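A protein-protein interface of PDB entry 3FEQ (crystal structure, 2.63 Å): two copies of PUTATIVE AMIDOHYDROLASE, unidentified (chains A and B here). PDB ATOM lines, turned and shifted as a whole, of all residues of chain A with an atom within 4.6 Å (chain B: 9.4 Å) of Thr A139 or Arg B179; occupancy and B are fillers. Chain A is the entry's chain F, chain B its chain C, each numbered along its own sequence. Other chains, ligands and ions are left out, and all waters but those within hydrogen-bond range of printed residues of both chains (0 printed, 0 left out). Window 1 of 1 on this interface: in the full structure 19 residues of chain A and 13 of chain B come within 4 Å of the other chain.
The guanidinium group (NH1) of Arg B179 is in salt-bridge range of the side-chain carboxylate (OD1) of Asp A169 (2.6 Å).
The guanidinium group of Arg B179 lies within salt-bridge range of the side-chain carboxylate of Glu A213, 3.1 Å away.
The backbone carbonyl oxygen (O) of Arg A146 lies within hydrogen-bond range of the side-chain amide nitrogen (NE2) of Gln B183, at 2.9 Å.
The side-chain amide oxygen of Gln B183 lies close to the side-chain carboxylate of Glu A153 (3.5 Å).
The side-chain carboxylate (OE2) of Glu B172 is in salt-bridge range of the guanidinium group (NE) of Arg B175.
OE1 of Glu B220 is in salt-bridge range of NE of Arg B179, 2.8 Å away.
The side-chain hydroxyl (OG1) of Thr A139 is in hydrogen-bond range of the side-chain carboxylate (OD2) of Asp A169 (2.8 Å).
The backbone NH (N) of Gly A140 lies within hydrogen-bond range of the side-chain carboxylate (OD2) of Asp A144 (2.6 Å).
OD1 of Asp A144 lies within salt-bridge range of NE of Arg A146, at 2.9 Å.
The backbone NH (N) of Ser A210 sits at hydrogen-bond distance from the side-chain carboxylate (OE2) of Glu A213.
CD of Arg B179 touches NE2 of Gln A138, 3.4 Å away.
Thr A139 touches Leu B176 (OG1 to CD1, 3.5 Å).
Thr A139 touches Arg B179 (O to CB, 3.6 Å).
Gln B183 touches Gly A140 (CG to CA, 3.5 Å).
Lys B184 touches Glu A153.
Asp A169 touches Leu B176.
NH2 of Arg B179 touches CA of Tyr A209, at 3.8 Å.
Ser A210 touches Arg B175 (CB to NH2, 3.7 Å).
Ser A210 touches Arg B179.
OE2 of Glu A213 touches CD of Arg B175, 3.9 Å away.
Gln A138 touches one residue of chain B.
Printed residues of chain B within 4 Å of Gly A140: Gln B183 (3.5 Å).
Of the printed residues of chain A, Gln B183 touches Gly A140, Arg A146 and Glu A153.
Of the printed residues of chain B, Asp A169 touches Leu B176 (3.7 Å) and Arg B179 (2.6 Å).
Of the printed residues of chain A, Leu B176 touches Thr A139 and Asp A169.
Glu B181 touches none of the printed residues of chain A.
Val B178 touches none of the printed residues of chain A.
The nearest residue of chain B that does not touch Thr A139 is Glu B180 (4.3 Å).
Hydrophobic or aromatic side chains of chain B that line the printed part of chain A: Leu B176.
No position is printed for both chains.
Of the 15 pairs that touch across the chains among the printed residues, none has its exchanged pair printed and touching as well.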
ATOM      1  N   SER A 137     -31.802  -4.829  12.680  1.00  0.00           N
ATOM      2  CA  SER A 137     -31.459  -5.130  14.078  1.00  0.00           C
ATOM      3  C   SER A 137     -30.683  -3.979  14.710  1.00  0.00           C
ATOM      4  O   SER A 137     -29.814  -3.380  14.068  1.00  0.00           O
ATOM      5  CB  SER A 137     -30.648  -6.415  14.166  1.00  0.00           C
ATOM      6  OG  SER A 137     -29.990  -6.509  15.409  1.00  0.00           O
ATOM      7  N   GLN A 138     -31.043  -3.632  15.942  1.00  0.00           N
ATOM      8  CA  GLN A 138     -30.350  -2.577  16.685  1.00  0.00           C
ATOM      9  C   GLN A 138     -29.020  -3.147  17.136  1.00  0.00           C
ATOM     10  O   GLN A 138     -28.781  -4.338  17.017  1.00  0.00           O
ATOM     11  CB  GLN A 138     -31.153  -2.149  17.922  1.00  0.00           C
ATOM     12  CG  GLN A 138     -31.388  -3.303  18.870  1.00  0.00           C
ATOM     13  CD  GLN A 138     -31.501  -2.885  20.289  1.00  0.00           C
ATOM     14  OE1 GLN A 138     -32.557  -2.446  20.738  1.00  0.00           O
ATOM     15  NE2 GLN A 138     -30.420  -3.052  21.031  1.00  0.00           N
ATOM     16  N   THR A 139     -28.171  -2.293  17.686  1.00  0.00           N
ATOM     17  CA  THR A 139     -26.856  -2.720  18.117  1.00  0.00           C
ATOM     18  C   THR A 139     -27.002  -3.628  19.326  1.00  0.00           C
ATOM     19  O   THR A 139     -27.753  -3.334  20.253  1.00  0.00           O
ATOM     20  CB  THR A 139     -25.962  -1.508  18.442  1.00  0.00           C
ATOM     21  OG1 THR A 139     -25.641  -0.816  17.228  1.00  0.00           O
ATOM     22  CG2 THR A 139     -24.677  -1.948  19.107  1.00  0.00           C
ATOM     23  N   GLY A 140     -26.310  -4.758  19.295  1.00  0.00           N
ATOM     24  CA  GLY A 140     -26.377  -5.705  20.393  1.00  0.00           C
ATOM     25  C   GLY A 140     -27.699  -6.429  20.358  1.00  0.00           C
ATOM     26  O   GLY A 140     -28.123  -7.032  21.341  1.00  0.00           O
ATOM     27  N   GLY A 141     -28.354  -6.351  19.211  1.00  0.00           N
ATOM     28  CA  GLY A 141     -29.664  -6.941  19.048  1.00  0.00           C
ATOM     29  C   GLY A 141     -29.536  -8.340  18.507  1.00  0.00           C
ATOM     30  O   GLY A 141     -28.425  -8.878  18.401  1.00  0.00           O
ATOM     31  N   ASP A 144     -27.188  -8.764  15.636  1.00  0.00           N
ATOM     32  CA  ASP A 144     -25.819  -8.331  15.858  1.00  0.00           C
ATOM     33  C   ASP A 144     -25.040  -9.563  16.317  1.00  0.00           C
ATOM     34  O   ASP A 144     -25.383 -10.172  17.330  1.00  0.00           O
ATOM     35  CB  ASP A 144     -25.796  -7.241  16.936  1.00  0.00           C
ATOM     36  CG  ASP A 144     -24.479  -6.466  16.972  1.00  0.00           C
ATOM     37  OD1 ASP A 144     -23.487  -6.917  16.353  1.00  0.00           O
ATOM     38  OD2 ASP A 144     -24.435  -5.404  17.633  1.00  0.00           O
ATOM     39  N   ARG A 146     -21.596  -9.830  16.779  1.00  0.00           N
ATOM     40  CA  ARG A 146     -20.307  -9.555  17.373  1.00  0.00           C
ATOM     41  C   ARG A 146     -20.239 -10.061  18.816  1.00  0.00           C
ATOM     42  O   ARG A 146     -21.231 -10.024  19.544  1.00  0.00           O
ATOM     43  CB  ARG A 146     -20.004  -8.065  17.256  1.00  0.00           C
ATOM     44  CG  ARG A 146     -19.968  -7.604  15.791  1.00  0.00           C
ATOM     45  CD  ARG A 146     -19.798  -6.107  15.662  1.00  0.00           C
ATOM     46  NE  ARG A 146     -21.036  -5.400  15.961  1.00  0.00           N
ATOM     47  CZ  ARG A 146     -21.184  -4.086  15.871  1.00  0.00           C
ATOM     48  NH1 ARG A 146     -20.156  -3.326  15.513  1.00  0.00           N
ATOM     49  NH2 ARG A 146     -22.361  -3.530  16.141  1.00  0.00           N
ATOM     50  N   GLU A 153     -16.316  -2.848  19.527  1.00  0.00           N
ATOM     51  CA  GLU A 153     -16.707  -3.330  18.186  1.00  0.00           C
ATOM     52  C   GLU A 153     -16.552  -2.284  17.080  1.00  0.00           C
ATOM     53  O   GLU A 153     -17.100  -1.184  17.185  1.00  0.00           O
ATOM     54  CB  GLU A 153     -18.160  -3.845  18.186  1.00  0.00           C
ATOM     55  CG  GLU A 153     -18.819  -3.987  19.554  1.00  0.00           C
ATOM     56  CD  GLU A 153     -19.277  -2.653  20.129  1.00  0.00           C
ATOM     57  OE1 GLU A 153     -18.439  -1.734  20.254  1.00  0.00           O
ATOM     58  OE2 GLU A 153     -20.469  -2.522  20.476  1.00  0.00           O
ATOM     59  N   VAL A 167     -27.094  -4.002  10.985  1.00  0.00           N
ATOM     60  CA  VAL A 167     -27.253  -3.252  12.213  1.00  0.00           C
ATOM     61  C   VAL A 167     -27.510  -1.778  11.927  1.00  0.00           C
ATOM     62  O   VAL A 167     -26.662  -1.095  11.335  1.00  0.00           O
ATOM     63  CB  VAL A 167     -26.032  -3.406  13.122  1.00  0.00           C
ATOM     64  CG1 VAL A 167     -26.278  -2.690  14.446  1.00  0.00           C
ATOM     65  CG2 VAL A 167     -25.749  -4.870  13.350  1.00  0.00           C
ATOM     66  N   ASP A 169     -29.379   1.802  13.840  1.00  0.00           N
ATOM     67  CA  ASP A 169     -29.988   2.414  15.009  1.00  0.00           C
ATOM     68  C   ASP A 169     -30.500   3.799  14.665  1.00  0.00           C
ATOM     69  O   ASP A 169     -29.979   4.445  13.758  1.00  0.00           O
ATOM     70  CB  ASP A 169     -28.993   2.493  16.166  1.00  0.00           C
ATOM     71  CG  ASP A 169     -28.352   1.150  16.481  1.00  0.00           C
ATOM     72  OD1 ASP A 169     -28.816   0.462  17.423  1.00  0.00           O
ATOM     73  OD2 ASP A 169     -27.385   0.785  15.775  1.00  0.00           O
ATOM     74  N   GLY A 170     -31.551   4.223  15.367  1.00  0.00           N
ATOM     75  CA  GLY A 170     -32.077   5.573  15.239  1.00  0.00           C
ATOM     76  C   GLY A 170     -33.231   5.673  14.279  1.00  0.00           C
ATOM     77  O   GLY A 170     -33.332   4.889  13.339  1.00  0.00           O
ATOM     78  N   TYR A 209     -35.279  -2.026  19.895  1.00  0.00           N
ATOM     79  CA  TYR A 209     -35.794  -0.849  19.180  1.00  0.00           C
ATOM     80  C   TYR A 209     -36.779  -0.011  19.995  1.00  0.00           C
ATOM     81  O   TYR A 209     -37.667  -0.538  20.682  1.00  0.00           O
ATOM     82  CB  TYR A 209     -36.427  -1.222  17.838  1.00  0.00           C
ATOM     83  CG  TYR A 209     -35.435  -1.458  16.723  1.00  0.00           C
ATOM     84  CD1 TYR A 209     -35.523  -2.590  15.914  1.00  0.00           C
ATOM     85  CD2 TYR A 209     -34.426  -0.537  16.464  1.00  0.00           C
ATOM     86  CE1 TYR A 209     -34.618  -2.803  14.887  1.00  0.00           C
ATOM     87  CE2 TYR A 209     -33.531  -0.733  15.440  1.00  0.00           C
ATOM     88  CZ  TYR A 209     -33.624  -1.871  14.662  1.00  0.00           C
ATOM     89  OH  TYR A 209     -32.721  -2.054  13.651  1.00  0.00           O
ATOM     90  N   SER A 210     -36.633   1.304  19.898  1.00  0.00           N
ATOM     91  CA  SER A 210     -37.566   2.201  20.551  1.00  0.00           C
ATOM     92  C   SER A 210     -38.918   2.157  19.823  1.00  0.00           C
ATOM     93  O   SER A 210     -39.008   1.662  18.686  1.00  0.00           O
ATOM     94  CB  SER A 210     -37.001   3.617  20.597  1.00  0.00           C
ATOM     95  OG  SER A 210     -36.966   4.172  19.299  1.00  0.00           O
ATOM     96  N   GLU A 213     -38.598   4.107  16.769  1.00  0.00           N
ATOM     97  CA  GLU A 213     -37.903   3.504  15.633  1.00  0.00           C
ATOM     98  C   GLU A 213     -38.848   2.580  14.885  1.00  0.00           C
ATOM     99  O   GLU A 213     -39.007   2.702  13.664  1.00  0.00           O
ATOM    100  CB  GLU A 213     -36.619   2.769  16.052  1.00  0.00           C
ATOM    101  CG  GLU A 213     -35.487   3.686  16.492  1.00  0.00           C
ATOM    102  CD  GLU A 213     -34.398   2.943  17.256  1.00  0.00           C
ATOM    103  OE1 GLU A 213     -33.306   2.729  16.691  1.00  0.00           O
ATOM    104  OE2 GLU A 213     -34.626   2.539  18.412  1.00  0.00           O
ATOM    105  N   LEU B 136     -21.781   7.823  30.875  1.00  0.00           N
ATOM    106  CA  LEU B 136     -22.148   8.736  29.811  1.00  0.00           C
ATOM    107  C   LEU B 136     -22.071  10.185  30.281  1.00  0.00           C
ATOM    108  O   LEU B 136     -22.446  10.494  31.401  1.00  0.00           O
ATOM    109  CB  LEU B 136     -23.533   8.401  29.303  1.00  0.00           C
ATOM    110  CG  LEU B 136     -23.671   6.973  28.789  1.00  0.00           C
ATOM    111  CD1 LEU B 136     -25.013   6.847  28.088  1.00  0.00           C
ATOM    112  CD2 LEU B 136     -22.530   6.608  27.852  1.00  0.00           C
ATOM    113  N   ARG B 166     -17.295   8.437  28.854  1.00  0.00           N
ATOM    114  CA  ARG B 166     -17.241   8.842  27.449  1.00  0.00           C
ATOM    115  C   ARG B 166     -18.156  10.057  27.185  1.00  0.00           C
ATOM    116  O   ARG B 166     -19.188  10.239  27.834  1.00  0.00           O
ATOM    117  CB  ARG B 166     -17.675   7.675  26.556  1.00  0.00           C
ATOM    118  CG  ARG B 166     -19.010   7.038  26.965  1.00  0.00           C
ATOM    119  CD  ARG B 166     -19.336   5.802  26.131  1.00  0.00           C
ATOM    120  NE  ARG B 166     -19.389   6.102  24.704  1.00  0.00           N
ATOM    121  CZ  ARG B 166     -19.845   5.260  23.779  1.00  0.00           C
ATOM    122  NH1 ARG B 166     -20.293   4.057  24.120  1.00  0.00           N
ATOM    123  NH2 ARG B 166     -19.870   5.629  22.511  1.00  0.00           N
ATOM    124  N   VAL B 171     -29.880  12.602  21.213  1.00  0.00           N
ATOM    125  CA  VAL B 171     -30.802  11.530  21.538  1.00  0.00           C
ATOM    126  C   VAL B 171     -30.411  10.230  20.888  1.00  0.00           C
ATOM    127  O   VAL B 171     -30.437   9.190  21.532  1.00  0.00           O
ATOM    128  CB  VAL B 171     -32.227  11.865  21.111  1.00  0.00           C
ATOM    129  CG1 VAL B 171     -33.082  10.631  21.164  1.00  0.00           C
ATOM    130  CG2 VAL B 171     -32.789  12.966  22.000  1.00  0.00           C
ATOM    131  N   GLU B 172     -30.057  10.270  19.611  1.00  0.00           N
ATOM    132  CA  GLU B 172     -29.624   9.055  18.960  1.00  0.00           C
ATOM    133  C   GLU B 172     -28.252   8.648  19.485  1.00  0.00           C
ATOM    134  O   GLU B 172     -27.982   7.462  19.682  1.00  0.00           O
ATOM    135  CB  GLU B 172     -29.621   9.207  17.439  1.00  0.00           C
ATOM    136  CG  GLU B 172     -30.984   9.585  16.842  1.00  0.00           C
ATOM    137  CD  GLU B 172     -32.073   8.510  17.022  1.00  0.00           C
ATOM    138  OE1 GLU B 172     -33.130   8.619  16.364  1.00  0.00           O
ATOM    139  OE2 GLU B 172     -31.885   7.556  17.814  1.00  0.00           O
ATOM    140  N   GLY B 173     -27.426   9.643  19.786  1.00  0.00           N
ATOM    141  CA  GLY B 173     -26.071   9.393  20.218  1.00  0.00           C
ATOM    142  C   GLY B 173     -26.073   8.589  21.492  1.00  0.00           C
ATOM    143  O   GLY B 173     -25.385   7.555  21.581  1.00  0.00           O
ATOM    144  N   VAL B 174     -26.883   9.033  22.456  1.00  0.00           N
ATOM    145  CA  VAL B 174     -26.943   8.352  23.740  1.00  0.00           C
ATOM    146  C   VAL B 174     -27.569   6.972  23.564  1.00  0.00           C
ATOM    147  O   VAL B 174     -27.144   5.987  24.194  1.00  0.00           O
ATOM    148  CB  VAL B 174     -27.656   9.179  24.838  1.00  0.00           C
ATOM    149  CG1 VAL B 174     -26.869  10.441  25.160  1.00  0.00           C
ATOM    150  CG2 VAL B 174     -29.093   9.518  24.458  1.00  0.00           C
ATOM    151  N   ARG B 175     -28.501   6.879  22.624  1.00  0.00           N
ATOM    152  CA  ARG B 175     -29.274   5.649  22.453  1.00  0.00           C
ATOM    153  C   ARG B 175     -28.318   4.570  22.013  1.00  0.00           C
ATOM    154  O   ARG B 175     -28.241   3.508  22.627  1.00  0.00           O
ATOM    155  CB  ARG B 175     -30.350   5.829  21.380  1.00  0.00           C
ATOM    156  CG  ARG B 175     -31.731   5.378  21.810  1.00  0.00           C
ATOM    157  CD  ARG B 175     -32.578   4.954  20.629  1.00  0.00           C
ATOM    158  NE  ARG B 175     -33.315   6.052  20.007  1.00  0.00           N
ATOM    159  CZ  ARG B 175     -34.372   6.664  20.545  1.00  0.00           C
ATOM    160  NH1 ARG B 175     -35.002   7.624  19.874  1.00  0.00           N
ATOM    161  NH2 ARG B 175     -34.785   6.342  21.757  1.00  0.00           N
ATOM    162  N   LEU B 176     -27.591   4.876  20.937  1.00  0.00           N
ATOM    163  CA  LEU B 176     -26.496   4.071  20.459  1.00  0.00           C
ATOM    164  C   LEU B 176     -25.459   3.787  21.548  1.00  0.00           C
ATOM    165  O   LEU B 176     -25.146   2.622  21.808  1.00  0.00           O
ATOM    166  CB  LEU B 176     -25.853   4.739  19.250  1.00  0.00           C
ATOM    167  CG  LEU B 176     -24.732   3.943  18.597  1.00  0.00           C
ATOM    168  CD1 LEU B 176     -25.241   2.586  18.137  1.00  0.00           C
ATOM    169  CD2 LEU B 176     -24.194   4.739  17.442  1.00  0.00           C
ATOM    170  N   ALA B 177     -24.984   4.811  22.252  1.00  0.00           N
ATOM    171  CA  ALA B 177     -24.026   4.521  23.344  1.00  0.00           C
ATOM    172  C   ALA B 177     -24.532   3.537  24.402  1.00  0.00           C
ATOM    173  O   ALA B 177     -23.772   2.681  24.851  1.00  0.00           O
ATOM    174  CB  ALA B 177     -23.508   5.773  23.983  1.00  0.00           C
ATOM    175  N   VAL B 178     -25.804   3.649  24.800  1.00  0.00           N
ATOM    176  CA  VAL B 178     -26.385   2.685  25.740  1.00  0.00           C
ATOM    177  C   VAL B 178     -26.376   1.259  25.149  1.00  0.00           C
ATOM    178  O   VAL B 178     -25.879   0.335  25.783  1.00  0.00           O
ATOM    179  CB  VAL B 178     -27.822   3.090  26.209  1.00  0.00           C
ATOM    180  CG1 VAL B 178     -28.440   2.001  27.029  1.00  0.00           C
ATOM    181  CG2 VAL B 178     -27.798   4.329  27.060  1.00  0.00           C
ATOM    182  N   ARG B 179     -26.902   1.076  23.937  1.00  0.00           N
ATOM    183  CA  ARG B 179     -26.839  -0.227  23.273  1.00  0.00           C
ATOM    184  C   ARG B 179     -25.391  -0.767  23.186  1.00  0.00           C
ATOM    185  O   ARG B 179     -25.144  -1.927  23.463  1.00  0.00           O
ATOM    186  CB  ARG B 179     -27.480  -0.164  21.879  1.00  0.00           C
ATOM    187  CG  ARG B 179     -28.922   0.247  21.909  1.00  0.00           C
ATOM    188  CD  ARG B 179     -29.569   0.250  20.542  1.00  0.00           C
ATOM    189  NE  ARG B 179     -30.971   0.693  20.601  1.00  0.00           N
ATOM    190  CZ  ARG B 179     -31.644   1.241  19.586  1.00  0.00           C
ATOM    191  NH1 ARG B 179     -31.071   1.408  18.397  1.00  0.00           N
ATOM    192  NH2 ARG B 179     -32.911   1.604  19.750  1.00  0.00           N
ATOM    193  N   GLU B 180     -24.436   0.091  22.850  1.00  0.00           N
ATOM    194  CA  GLU B 180     -23.040  -0.309  22.809  1.00  0.00           C
ATOM    195  C   GLU B 180     -22.598  -0.816  24.161  1.00  0.00           C
ATOM    196  O   GLU B 180     -21.902  -1.835  24.250  1.00  0.00           O
ATOM    197  CB  GLU B 180     -22.137   0.860  22.387  1.00  0.00           C
ATOM    198  CG  GLU B 180     -22.171   1.208  20.894  1.00  0.00           C
ATOM    199  CD  GLU B 180     -21.542   2.563  20.580  1.00  0.00           C
ATOM    200  OE1 GLU B 180     -21.389   2.891  19.380  1.00  0.00           O
ATOM    201  OE2 GLU B 180     -21.204   3.305  21.530  1.00  0.00           O
ATOM    202  N   GLU B 181     -22.995  -0.097  25.212  1.00  0.00           N
ATOM    203  CA  GLU B 181     -22.494  -0.379  26.561  1.00  0.00           C
ATOM    204  C   GLU B 181     -23.071  -1.676  27.080  1.00  0.00           C
ATOM    205  O   GLU B 181     -22.375  -2.496  27.659  1.00  0.00           O
ATOM    206  CB  GLU B 181     -22.792   0.766  27.529  1.00  0.00           C
ATOM    207  CG  GLU B 181     -21.854   1.988  27.393  1.00  0.00           C
ATOM    208  CD  GLU B 181     -20.362   1.657  27.187  1.00  0.00           C
ATOM    209  OE1 GLU B 181     -19.817   0.784  27.898  1.00  0.00           O
ATOM    210  OE2 GLU B 181     -19.724   2.327  26.342  1.00  0.00           O
ATOM    211  N   ILE B 182     -24.332  -1.900  26.768  1.00  0.00           N
ATOM    212  CA  ILE B 182     -24.988  -3.138  27.123  1.00  0.00           C
ATOM    213  C   ILE B 182     -24.462  -4.326  26.328  1.00  0.00           C
ATOM    214  O   ILE B 182     -24.234  -5.394  26.896  1.00  0.00           O
ATOM    215  CB  ILE B 182     -26.513  -2.980  27.025  1.00  0.00           C
ATOM    216  CG1 ILE B 182     -27.021  -2.426  28.342  1.00  0.00           C
ATOM    217  CG2 ILE B 182     -27.199  -4.304  26.738  1.00  0.00           C
ATOM    218  CD1 ILE B 182     -27.954  -1.264  28.184  1.00  0.00           C
ATOM    219  N   GLN B 183     -24.245  -4.147  25.027  1.00  0.00           N
ATOM    220  CA  GLN B 183     -23.579  -5.189  24.249  1.00  0.00           C
ATOM    221  C   GLN B 183     -22.218  -5.545  24.851  1.00  0.00           C
ATOM    222  O   GLN B 183     -21.938  -6.722  25.041  1.00  0.00           O
ATOM    223  CB  GLN B 183     -23.458  -4.828  22.771  1.00  0.00           C
ATOM    224  CG  GLN B 183     -23.192  -6.033  21.873  1.00  0.00           C
ATOM    225  CD  GLN B 183     -21.700  -6.359  21.682  1.00  0.00           C
ATOM    226  OE1 GLN B 183     -20.815  -5.580  22.055  1.00  0.00           O
ATOM    227  NE2 GLN B 183     -21.426  -7.520  21.090  1.00  0.00           N
ATOM    228  N   LYS B 184     -21.420  -4.540  25.224  1.00  0.00           N
ATOM    229  CA  LYS B 184     -20.126  -4.802  25.845  1.00  0.00           C
ATOM    230  C   LYS B 184     -20.243  -5.458  27.220  1.00  0.00           C
ATOM    231  O   LYS B 184     -19.248  -5.947  27.766  1.00  0.00           O
ATOM    232  CB  LYS B 184     -19.289  -3.529  25.956  1.00  0.00           C
ATOM    233  CG  LYS B 184     -18.796  -2.970  24.638  1.00  0.00           C
ATOM    234  CD  LYS B 184     -17.874  -1.794  24.903  1.00  0.00           C
ATOM    235  CE  LYS B 184     -18.103  -0.665  23.928  1.00  0.00           C
ATOM    236  NZ  LYS B 184     -17.802   0.649  24.575  1.00  0.00           N
ATOM    237  N   GLY B 185     -21.437  -5.425  27.802  1.00  0.00           N
ATOM    238  CA  GLY B 185     -21.716  -6.218  28.999  1.00  0.00           C
ATOM    239  C   GLY B 185     -21.899  -5.476  30.318  1.00  0.00           C
ATOM    240  O   GLY B 185     -21.778  -6.067  31.384  1.00  0.00           O
ATOM    241  N   ALA B 186     -22.233  -4.193  30.248  1.00  0.00           N
ATOM    242  CA  ALA B 186     -22.662  -3.418  31.425  1.00  0.00           C
ATOM    243  C   ALA B 186     -23.853  -4.059  32.123  1.00  0.00           C
ATOM    244  O   ALA B 186     -24.709  -4.630  31.477  1.00  0.00           O
ATOM    245  CB  ALA B 186     -23.016  -1.988  31.014  1.00  0.00           C
ATOM    246  N   ILE B 189     -26.486   1.333  33.688  1.00  0.00           N
ATOM    247  CA  ILE B 189     -25.960   2.465  32.947  1.00  0.00           C
ATOM    248  C   ILE B 189     -25.766   3.645  33.863  1.00  0.00           C
ATOM    249  O   ILE B 189     -26.674   3.965  34.617  1.00  0.00           O
ATOM    250  CB  ILE B 189     -26.902   2.874  31.823  1.00  0.00           C
ATOM    251  CG1 ILE B 189     -27.086   1.723  30.814  1.00  0.00           C
ATOM    252  CG2 ILE B 189     -26.388   4.133  31.153  1.00  0.00           C
ATOM    253  CD1 ILE B 189     -25.792   1.307  30.096  1.00  0.00           C
ATOM    254  N   ALA B 216     -34.408   8.923  26.765  1.00  0.00           N
ATOM    255  CA  ALA B 216     -33.945   7.912  25.792  1.00  0.00           C
ATOM    256  C   ALA B 216     -33.014   6.878  26.443  1.00  0.00           C
ATOM    257  O   ALA B 216     -33.210   5.677  26.278  1.00  0.00           O
ATOM    258  CB  ALA B 216     -33.286   8.567  24.585  1.00  0.00           C
ATOM    259  N   ILE B 217     -32.084   7.364  27.267  1.00  0.00           N
ATOM    260  CA  ILE B 217     -31.142   6.536  28.046  1.00  0.00           C
ATOM    261  C   ILE B 217     -31.834   5.547  28.962  1.00  0.00           C
ATOM    262  O   ILE B 217     -31.447   4.377  29.041  1.00  0.00           O
ATOM    263  CB  ILE B 217     -30.226   7.432  28.942  1.00  0.00           C
ATOM    264  CG1 ILE B 217     -29.283   8.269  28.098  1.00  0.00           C
ATOM    265  CG2 ILE B 217     -29.445   6.621  29.944  1.00  0.00           C
ATOM    266  CD1 ILE B 217     -28.719   9.417  28.856  1.00  0.00           C
ATOM    267  N   ASP B 219     -34.972   4.477  28.746  1.00  0.00           N
ATOM    268  CA  ASP B 219     -35.672   3.499  27.915  1.00  0.00           C
ATOM    269  C   ASP B 219     -34.754   2.373  27.453  1.00  0.00           C
ATOM    270  O   ASP B 219     -35.065   1.209  27.636  1.00  0.00           O
ATOM    271  CB  ASP B 219     -36.332   4.161  26.700  1.00  0.00           C
ATOM    272  CG  ASP B 219     -37.436   5.146  27.084  1.00  0.00           C
ATOM    273  OD1 ASP B 219     -37.847   5.170  28.266  1.00  0.00           O
ATOM    274  OD2 ASP B 219     -37.895   5.902  26.193  1.00  0.00           O
ATOM    275  N   GLU B 220     -33.611   2.721  26.878  1.00  0.00           N
ATOM    276  CA  GLU B 220     -32.697   1.712  26.361  1.00  0.00           C
ATOM    277  C   GLU B 220     -32.180   0.795  27.462  1.00  0.00           C
ATOM    278  O   GLU B 220     -32.078  -0.427  27.284  1.00  0.00           O
ATOM    279  CB  GLU B 220     -31.548   2.374  25.633  1.00  0.00           C
ATOM    280  CG  GLU B 220     -31.986   3.094  24.389  1.00  0.00           C
ATOM    281  CD  GLU B 220     -32.674   2.172  23.405  1.00  0.00           C
ATOM    282  OE1 GLU B 220     -32.126   1.073  23.121  1.00  0.00           O
ATOM    283  OE2 GLU B 220     -33.766   2.553  22.929  1.00  0.00           O
ATOM    284  N   ALA B 221     -31.926   1.375  28.627  1.00  0.00           N
ATOM    285  CA  ALA B 221     -31.596   0.571  29.793  1.00  0.00           C
ATOM    286  C   ALA B 221     -32.738  -0.374  30.205  1.00  0.00           C
ATOM    287  O   ALA B 221     -32.497  -1.545  30.525  1.00  0.00           O
ATOM    288  CB  ALA B 221     -31.190   1.464  30.938  1.00  0.00           C
ATOM    289  N   ALA B 223     -35.229  -1.451  28.269  1.00  0.00           N
ATOM    290  CA  ALA B 223     -35.333  -2.452  27.225  1.00  0.00           C
ATOM    291  C   ALA B 223     -34.363  -3.617  27.470  1.00  0.00           C
ATOM    292  O   ALA B 223     -34.657  -4.734  27.084  1.00  0.00           O
ATOM    293  CB  ALA B 223     -35.095  -1.822  25.861  1.00  0.00           C
ATOM    294  N   ALA B 224     -33.231  -3.362  28.132  1.00  0.00           N
ATOM    295  CA  ALA B 224     -32.263  -4.415  28.442  1.00  0.00           C
ATOM    296  C   ALA B 224     -32.418  -4.944  29.866  1.00  0.00           C
ATOM    297  O   ALA B 224     -31.497  -5.558  30.431  1.00  0.00           O
ATOM    298  CB  ALA B 224     -30.814  -3.923  28.201  1.00  0.00           C
